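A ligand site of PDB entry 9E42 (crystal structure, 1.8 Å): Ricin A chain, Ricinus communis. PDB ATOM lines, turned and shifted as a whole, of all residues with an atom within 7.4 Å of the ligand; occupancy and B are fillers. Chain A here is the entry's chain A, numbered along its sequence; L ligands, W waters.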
ATOM      1  N   TYR A 187      31.755 -31.016   3.780  1.00  0.00           N
ATOM      2  CA  TYR A 187      31.907 -30.731   5.197  1.00  0.00           C
ATOM      3  C   TYR A 187      32.776 -31.776   5.882  1.00  0.00           C
ATOM      4  O   TYR A 187      33.645 -31.441   6.693  1.00  0.00           O
ATOM      5  CB  TYR A 187      30.530 -30.673   5.860  1.00  0.00           C
ATOM      6  CG  TYR A 187      30.542 -30.284   7.325  1.00  0.00           C
ATOM      7  CD1 TYR A 187      30.614 -28.956   7.694  1.00  0.00           C
ATOM      8  CD2 TYR A 187      30.435 -31.246   8.322  1.00  0.00           C
ATOM      9  CE1 TYR A 187      30.609 -28.583   9.037  1.00  0.00           C
ATOM     10  CE2 TYR A 187      30.431 -30.887   9.666  1.00  0.00           C
ATOM     11  CZ  TYR A 187      30.516 -29.552  10.018  1.00  0.00           C
ATOM     12  OH  TYR A 187      30.509 -29.202  11.352  1.00  0.00           O
ATOM     13  N   GLU A 191      36.413 -31.769   7.573  1.00  0.00           N
ATOM     14  CA  GLU A 191      36.718 -32.306   8.904  1.00  0.00           C
ATOM     15  C   GLU A 191      37.999 -33.131   8.901  1.00  0.00           C
ATOM     16  O   GLU A 191      38.785 -33.055   9.859  1.00  0.00           O
ATOM     17  CB  GLU A 191      35.563 -33.175   9.398  1.00  0.00           C
ATOM     18  CG  GLU A 191      34.299 -32.427   9.755  1.00  0.00           C
ATOM     19  CD  GLU A 191      34.404 -31.726  11.092  1.00  0.00           C
ATOM     20  OE1 GLU A 191      35.029 -32.293  12.016  1.00  0.00           O
ATOM     21  OE2 GLU A 191      33.852 -30.617  11.224  1.00  0.00           O
ATOM     22  N   ASP A 205      32.288 -35.320  15.624  1.00  0.00           N
ATOM     23  CA  ASP A 205      31.337 -34.718  16.540  1.00  0.00           C
ATOM     24  C   ASP A 205      29.918 -34.890  16.000  1.00  0.00           C
ATOM     25  O   ASP A 205      29.722 -35.417  14.900  1.00  0.00           O
ATOM     26  CB  ASP A 205      31.709 -33.244  16.776  1.00  0.00           C
ATOM     27  CG  ASP A 205      31.517 -32.342  15.574  1.00  0.00           C
ATOM     28  OD1 ASP A 205      30.759 -32.664  14.631  1.00  0.00           O
ATOM     29  OD2 ASP A 205      32.106 -31.238  15.593  1.00  0.00           O
ATOM     30  N   PRO A 206      28.895 -34.503  16.775  1.00  0.00           N
ATOM     31  CA  PRO A 206      27.517 -34.780  16.345  1.00  0.00           C
ATOM     32  C   PRO A 206      27.139 -34.207  14.995  1.00  0.00           C
ATOM     33  O   PRO A 206      26.326 -34.812  14.284  1.00  0.00           O
ATOM     34  CB  PRO A 206      26.679 -34.165  17.480  1.00  0.00           C
ATOM     35  CG  PRO A 206      27.537 -34.328  18.656  1.00  0.00           C
ATOM     36  CD  PRO A 206      28.921 -34.021  18.171  1.00  0.00           C
ATOM     37  N   SER A 207      27.728 -33.078  14.586  1.00  0.00           N
ATOM     38  CA  SER A 207      27.381 -32.512  13.280  1.00  0.00           C
ATOM     39  C   SER A 207      27.806 -33.459  12.162  1.00  0.00           C
ATOM     40  O   SER A 207      27.104 -33.621  11.158  1.00  0.00           O
ATOM     41  CB  SER A 207      28.025 -31.144  13.099  1.00  0.00           C
ATOM     42  OG  SER A 207      29.426 -31.260  12.939  1.00  0.00           O
ATOM     43  N   VAL A 208      28.958 -34.107  12.331  1.00  0.00           N
ATOM     44  CA  VAL A 208      29.431 -35.063  11.338  1.00  0.00           C
ATOM     45  C   VAL A 208      28.572 -36.321  11.369  1.00  0.00           C
ATOM     46  O   VAL A 208      28.148 -36.828  10.315  1.00  0.00           O
ATOM     47  CB  VAL A 208      30.905 -35.402  11.588  1.00  0.00           C
ATOM     48  CG1 VAL A 208      31.400 -36.478  10.593  1.00  0.00           C
ATOM     49  CG2 VAL A 208      31.747 -34.135  11.518  1.00  0.00           C
ATOM     50  N   THR A 210      25.516 -36.834  12.495  1.00  0.00           N
ATOM     51  CA  THR A 210      24.138 -36.628  12.047  1.00  0.00           C
ATOM     52  C   THR A 210      24.075 -36.324  10.559  1.00  0.00           C
ATOM     53  O   THR A 210      23.116 -36.726   9.883  1.00  0.00           O
ATOM     54  CB  THR A 210      23.477 -35.545  12.888  1.00  0.00           C
ATOM     55  OG1 THR A 210      23.249 -36.053  14.211  1.00  0.00           O
ATOM     56  CG2 THR A 210      22.149 -35.105  12.286  1.00  0.00           C
ATOM     57  N   LEU A 211      25.080 -35.635  10.009  1.00  0.00           N
ATOM     58  CA  LEU A 211      25.158 -35.489   8.554  1.00  0.00           C
ATOM     59  C   LEU A 211      25.237 -36.845   7.878  1.00  0.00           C
ATOM     60  O   LEU A 211      24.503 -37.119   6.917  1.00  0.00           O
ATOM     61  CB  LEU A 211      26.376 -34.647   8.147  1.00  0.00           C
ATOM     62  CG  LEU A 211      26.150 -33.218   7.636  1.00  0.00           C
ATOM     63  CD1 LEU A 211      27.478 -32.653   7.190  1.00  0.00           C
ATOM     64  CD2 LEU A 211      25.137 -33.182   6.493  1.00  0.00           C
ATOM     65  N   LEU A 218      18.398 -36.272   3.248  1.00  0.00           N
ATOM     66  CA  LEU A 218      18.752 -35.015   2.606  1.00  0.00           C
ATOM     67  C   LEU A 218      18.658 -35.123   1.095  1.00  0.00           C
ATOM     68  O   LEU A 218      18.181 -34.201   0.420  1.00  0.00           O
ATOM     69  CB  LEU A 218      20.164 -34.581   3.021  1.00  0.00           C
ATOM     70  CG  LEU A 218      20.352 -34.079   4.440  1.00  0.00           C
ATOM     71  CD1 LEU A 218      21.820 -33.886   4.718  1.00  0.00           C
ATOM     72  CD2 LEU A 218      19.594 -32.762   4.627  1.00  0.00           C
ATOM     73  N   LEU A 236      19.138 -31.356  11.719  1.00  0.00           N
ATOM     74  CA  LEU A 236      20.556 -31.693  11.778  1.00  0.00           C
ATOM     75  C   LEU A 236      21.122 -31.207  13.107  1.00  0.00           C
ATOM     76  O   LEU A 236      20.471 -30.465  13.847  1.00  0.00           O
ATOM     77  CB  LEU A 236      21.317 -31.084  10.599  1.00  0.00           C
ATOM     78  CG  LEU A 236      20.812 -31.535   9.235  1.00  0.00           C
ATOM     79  CD1 LEU A 236      21.588 -30.822   8.135  1.00  0.00           C
ATOM     80  CD2 LEU A 236      20.921 -33.037   9.095  1.00  0.00           C
ATOM     81  N   GLN A 237      22.338 -31.634  13.414  1.00  0.00           N
ATOM     82  CA  GLN A 237      22.963 -31.315  14.684  1.00  0.00           C
ATOM     83  C   GLN A 237      24.095 -30.324  14.488  1.00  0.00           C
ATOM     84  O   GLN A 237      24.787 -30.349  13.466  1.00  0.00           O
ATOM     85  CB  GLN A 237      23.488 -32.565  15.387  1.00  0.00           C
ATOM     86  CG  GLN A 237      22.476 -33.214  16.324  1.00  0.00           C
ATOM     87  CD  GLN A 237      23.058 -34.399  17.062  1.00  0.00           C
ATOM     88  OE1 GLN A 237      23.488 -35.375  16.449  1.00  0.00           O
ATOM     89  NE2 GLN A 237      23.113 -34.303  18.380  1.00  0.00           N
ATOM     90  N   ARG A 238      24.251 -29.417  15.450  1.00  0.00           N
ATOM     91  CA  ARG A 238      25.424 -28.557  15.505  1.00  0.00           C
ATOM     92  C   ARG A 238      26.595 -29.303  16.138  1.00  0.00           C
ATOM     93  O   ARG A 238      26.466 -30.457  16.571  1.00  0.00           O
ATOM     94  CB  ARG A 238      25.100 -27.263  16.261  1.00  0.00           C
ATOM     95  CG  ARG A 238      23.893 -26.516  15.712  1.00  0.00           C
ATOM     96  CD  ARG A 238      23.740 -25.156  16.340  1.00  0.00           C
ATOM     97  NE  ARG A 238      22.669 -24.397  15.698  1.00  0.00           N
ATOM     98  CZ  ARG A 238      22.833 -23.626  14.635  1.00  0.00           C
ATOM     99  NH1 ARG A 238      24.008 -23.472  14.060  1.00  0.00           N
ATOM    100  NH2 ARG A 238      21.778 -22.984  14.139  1.00  0.00           N
ATOM    101  N   ARG A 239      27.768 -28.660  16.172  1.00  0.00           N
ATOM    102  CA  ARG A 239      28.930 -29.326  16.761  1.00  0.00           C
ATOM    103  C   ARG A 239      28.729 -29.584  18.239  1.00  0.00           C
ATOM    104  O   ARG A 239      29.268 -30.569  18.771  1.00  0.00           O
ATOM    105  CB  ARG A 239      30.189 -28.473  16.539  1.00  0.00           C
ATOM    106  CG  ARG A 239      30.610 -28.346  15.098  1.00  0.00           C
ATOM    107  CD  ARG A 239      31.947 -27.644  15.003  1.00  0.00           C
ATOM    108  NE  ARG A 239      32.279 -27.264  13.633  1.00  0.00           N
ATOM    109  CZ  ARG A 239      32.992 -28.000  12.797  1.00  0.00           C
ATOM    110  NH1 ARG A 239      33.446 -29.207  13.141  1.00  0.00           N
ATOM    111  NH2 ARG A 239      33.253 -27.527  11.584  1.00  0.00           N
ATOM    112  N   ASN A 240      27.979 -28.727  18.923  1.00  0.00           N
ATOM    113  CA  ASN A 240      27.694 -28.868  20.348  1.00  0.00           C
ATOM    114  C   ASN A 240      26.520 -29.801  20.630  1.00  0.00           C
ATOM    115  O   ASN A 240      26.120 -29.933  21.791  1.00  0.00           O
ATOM    116  CB  ASN A 240      27.453 -27.491  20.986  1.00  0.00           C
ATOM    117  CG  ASN A 240      26.281 -26.721  20.372  1.00  0.00           C
ATOM    118  OD1 ASN A 240      25.457 -27.273  19.631  1.00  0.00           O
ATOM    119  ND2 ASN A 240      26.204 -25.431  20.683  1.00  0.00           N
ATOM    120  N   GLY A 241      25.959 -30.449  19.607  1.00  0.00           N
ATOM    121  CA  GLY A 241      24.860 -31.374  19.797  1.00  0.00           C
ATOM    122  C   GLY A 241      23.473 -30.792  19.680  1.00  0.00           C
ATOM    123  O   GLY A 241      22.512 -31.545  19.518  1.00  0.00           O
ATOM    124  N   SER A 242      23.321 -29.469  19.780  1.00  0.00           N
ATOM    125  CA  SER A 242      22.011 -28.851  19.623  1.00  0.00           C
ATOM    126  C   SER A 242      21.524 -29.004  18.182  1.00  0.00           C
ATOM    127  O   SER A 242      22.304 -29.192  17.239  1.00  0.00           O
ATOM    128  CB  SER A 242      22.048 -27.380  20.008  1.00  0.00           C
ATOM    129  OG  SER A 242      22.930 -26.657  19.167  1.00  0.00           O
ATOM    130  N   PHE A 244      19.048 -27.919  14.732  1.00  0.00           N
ATOM    131  CA  PHE A 244      18.469 -26.846  13.953  1.00  0.00           C
ATOM    132  C   PHE A 244      17.760 -27.460  12.758  1.00  0.00           C
ATOM    133  O   PHE A 244      18.046 -28.596  12.377  1.00  0.00           O
ATOM    134  CB  PHE A 244      19.521 -25.812  13.512  1.00  0.00           C
ATOM    135  CG  PHE A 244      20.475 -26.330  12.471  1.00  0.00           C
ATOM    136  CD1 PHE A 244      21.536 -27.146  12.828  1.00  0.00           C
ATOM    137  CD2 PHE A 244      20.324 -25.969  11.138  1.00  0.00           C
ATOM    138  CE1 PHE A 244      22.418 -27.621  11.875  1.00  0.00           C
ATOM    139  CE2 PHE A 244      21.202 -26.439  10.172  1.00  0.00           C
ATOM    140  CZ  PHE A 244      22.253 -27.262  10.537  1.00  0.00           C
ATOM    141  N   VAL A 246      16.621 -27.523   8.751  1.00  0.00           N
ATOM    142  CA  VAL A 246      16.979 -27.140   7.391  1.00  0.00           C
ATOM    143  C   VAL A 246      15.699 -27.139   6.562  1.00  0.00           C
ATOM    144  O   VAL A 246      14.955 -28.122   6.562  1.00  0.00           O
ATOM    145  CB  VAL A 246      18.026 -28.097   6.788  1.00  0.00           C
ATOM    146  CG1 VAL A 246      18.289 -27.747   5.323  1.00  0.00           C
ATOM    147  CG2 VAL A 246      19.315 -28.022   7.591  1.00  0.00           C
ATOM    148  N   ILE A 251      21.096 -23.958   1.725  1.00  0.00           N
ATOM    149  CA  ILE A 251      22.053 -23.953   2.823  1.00  0.00           C
ATOM    150  C   ILE A 251      22.986 -25.164   2.771  1.00  0.00           C
ATOM    151  O   ILE A 251      24.049 -25.147   3.395  1.00  0.00           O
ATOM    152  CB  ILE A 251      21.341 -23.872   4.195  1.00  0.00           C
ATOM    153  CG1 ILE A 251      22.276 -23.255   5.234  1.00  0.00           C
ATOM    154  CG2 ILE A 251      20.900 -25.257   4.650  1.00  0.00           C
ATOM    155  CD1 ILE A 251      21.619 -23.031   6.578  1.00  0.00           C
ATOM    156  N   LEU A 252      22.623 -26.201   2.016  1.00  0.00           N
ATOM    157  CA  LEU A 252      23.397 -27.428   1.974  1.00  0.00           C
ATOM    158  C   LEU A 252      24.396 -27.470   0.826  1.00  0.00           C
ATOM    159  O   LEU A 252      25.215 -28.394   0.779  1.00  0.00           O
ATOM    160  CB  LEU A 252      22.462 -28.628   1.877  1.00  0.00           C
ATOM    161  CG  LEU A 252      21.497 -28.750   3.063  1.00  0.00           C
ATOM    162  CD1 LEU A 252      20.377 -29.720   2.730  1.00  0.00           C
ATOM    163  CD2 LEU A 252      22.230 -29.190   4.320  1.00  0.00           C
ATOM    164  N   ILE A 253      24.334 -26.503  -0.092  1.00  0.00           N
ATOM    165  CA  ILE A 253      25.223 -26.505  -1.260  1.00  0.00           C
ATOM    166  C   ILE A 253      26.695 -26.620  -0.875  1.00  0.00           C
ATOM    167  O   ILE A 253      27.412 -27.427  -1.479  1.00  0.00           O
ATOM    168  CB  ILE A 253      24.932 -25.292  -2.155  1.00  0.00           C
ATOM    169  CG1 ILE A 253      23.524 -25.399  -2.751  1.00  0.00           C
ATOM    170  CG2 ILE A 253      25.969 -25.191  -3.261  1.00  0.00           C
ATOM    171  CD1 ILE A 253      23.052 -24.124  -3.396  1.00  0.00           C
ATOM    172  N   PRO A 254      27.220 -25.839   0.080  1.00  0.00           N
ATOM    173  CA  PRO A 254      28.630 -26.022   0.472  1.00  0.00           C
ATOM    174  C   PRO A 254      28.879 -27.257   1.322  1.00  0.00           C
ATOM    175  O   PRO A 254      30.031 -27.492   1.715  1.00  0.00           O
ATOM    176  CB  PRO A 254      28.958 -24.740   1.254  1.00  0.00           C
ATOM    177  CG  PRO A 254      27.804 -23.807   1.024  1.00  0.00           C
ATOM    178  CD  PRO A 254      26.628 -24.697   0.790  1.00  0.00           C
ATOM    179  N   ILE A 255      27.846 -28.035   1.627  1.00  0.00           N
ATOM    180  CA  ILE A 255      27.929 -29.099   2.625  1.00  0.00           C
ATOM    181  C   ILE A 255      27.926 -30.471   1.977  1.00  0.00           C
ATOM    182  O   ILE A 255      28.762 -31.320   2.300  1.00  0.00           O
ATOM    183  CB  ILE A 255      26.776 -28.974   3.648  1.00  0.00           C
ATOM    184  CG1 ILE A 255      26.863 -27.634   4.393  1.00  0.00           C
ATOM    185  CG2 ILE A 255      26.758 -30.189   4.573  1.00  0.00           C
ATOM    186  CD1 ILE A 255      28.177 -27.438   5.128  1.00  0.00           C
ATOM    187  N   ILE A 256      26.981 -30.729   1.078  1.00  0.00           N
ATOM    188  CA  ILE A 256      26.807 -32.036   0.470  1.00  0.00           C
ATOM    189  C   ILE A 256      27.302 -31.969  -0.972  1.00  0.00           C
ATOM    190  O   ILE A 256      26.931 -31.056  -1.714  1.00  0.00           O
ATOM    191  CB  ILE A 256      25.345 -32.505   0.551  1.00  0.00           C
ATOM    192  CG1 ILE A 256      25.160 -33.831  -0.198  1.00  0.00           C
ATOM    193  CG2 ILE A 256      24.382 -31.430   0.043  1.00  0.00           C
ATOM    194  CD1 ILE A 256      23.824 -34.507   0.107  1.00  0.00           C
HETATM  195  C1  LIG L   1      25.600 -26.991   9.089  1.00  0.00           C
HETATM  196  C2  LIG L   1      28.103 -26.852  12.031  1.00  0.00           C
HETATM  197  C3  LIG L   1      26.522 -23.803   7.204  1.00  0.00           C
HETATM  198  C4  LIG L   1      26.252 -24.619   8.480  1.00  0.00           C
HETATM  199  C5  LIG L   1      25.536 -25.945   8.174  1.00  0.00           C
HETATM  200  C6  LIG L   1      24.835 -26.101   6.988  1.00  0.00           C
HETATM  201  C7  LIG L   1      24.179 -27.303   6.733  1.00  0.00           C
HETATM  202  C8  LIG L   1      24.249 -28.341   7.650  1.00  0.00           C
HETATM  203  C9  LIG L   1      24.953 -28.186   8.826  1.00  0.00           C
HETATM  204  C10 LIG L   1      25.010 -29.348   9.846  1.00  0.00           C
HETATM  205  C11 LIG L   1      26.205 -30.263   9.568  1.00  0.00           C
HETATM  206  C12 LIG L   1      26.374 -26.786  10.401  1.00  0.00           C
HETATM  207  C13 LIG L   1      27.681 -27.221  10.709  1.00  0.00           C
HETATM  208  C14 LIG L   1      27.147 -26.136  12.775  1.00  0.00           C
HETATM  209  C15 LIG L   1      27.283 -25.607  14.205  1.00  0.00           C
HETATM  210  O1  LIG L   1      26.557 -24.650  14.589  1.00  0.00           O
HETATM  211  O2  LIG L   1      28.121 -26.113  14.994  1.00  0.00           O
HETATM  212  S1  LIG L   1      25.797 -25.969  11.766  1.00  0.00           S
HETATM  213  O   HOH W   1      24.478 -32.084  11.726  1.00  0.00           O
HETATM  214  O   HOH W   2      28.193 -25.967  18.270  1.00  0.00           O
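The backbone NH (N) of Arg 239 sits at hydrogen-bond distance from an oxygen (O2) of the ligand (2.8 Å). An oxygen (O1) of the ligand is in salt-bridge range of the guanidinium group (NH1) of Arg 238 (2.9 Å).
The guanidinium group (NH2) of Arg 239 lies close to the side-chain hydroxyl (OH) of Tyr 187. The guanidinium group (NH1) of Arg 239 lies within salt-bridge range of the side-chain carboxylate (OD2) of Asp 205 (3.5 Å). The guanidinium group (NH1) of Arg 239 is in salt-bridge range of the side-chain carboxylate (OE2) of Glu 191, at 2.4 Å. O of Phe 244 lies within hydrogen-bond range of N of Leu 236, at 3.0 Å. N of Tyr 187 lies within hydrogen-bond range of O of Ile 255. The side-chain hydroxyl of Tyr 187 is in hydrogen-bond range of the side-chain hydroxyl of Ser 207 (2.8 Å). The backbone carbonyl oxygen (O) of Gly 241 sits at hydrogen-bond distance from the side-chain amide nitrogen (NE2) of Gln 237 (3.0 Å). OD1 of Asp 205 lies within hydrogen-bond range of OG of Ser 207, 2.6 Å away.
Tyr 187 touches the ligand (OH to C2, 3.4 Å). O of Ser 207 touches C11 of the ligand, at 3.8 Å. Leu 211 touches the ligand (CG to C11, 3.5 Å). Leu 236 touches the ligand (CD1 to C8, 3.7 Å). Gln 237 touches the ligand. CZ of Phe 244 touches C9 of the ligand (3.3 Å). Ile 251 touches the ligand. Leu 252 touches the ligand (CD2 to C7, 3.6 Å). Ile 255 touches the ligand (CG1 to C7, 3.6 Å). 11 residues have an atom within 4 Å of the ligand: Tyr 187, Ser 207, Leu 211, Leu 236, Gln 237, Arg 238, Arg 239, Phe 244, Ile 251, Leu 252 and Ile 255.
Water W2 lies within hydrogen-bond range of N of Asn 240 (2.8 Å), O2 of the ligand (3.3 Å) and N of Arg 239 (3.4 Å). Water W1 bridges the backbone carbonyl oxygen of Gln 237 (2.5 Å) and the backbone carbonyl oxygen of Ser 207 (3.1 Å).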
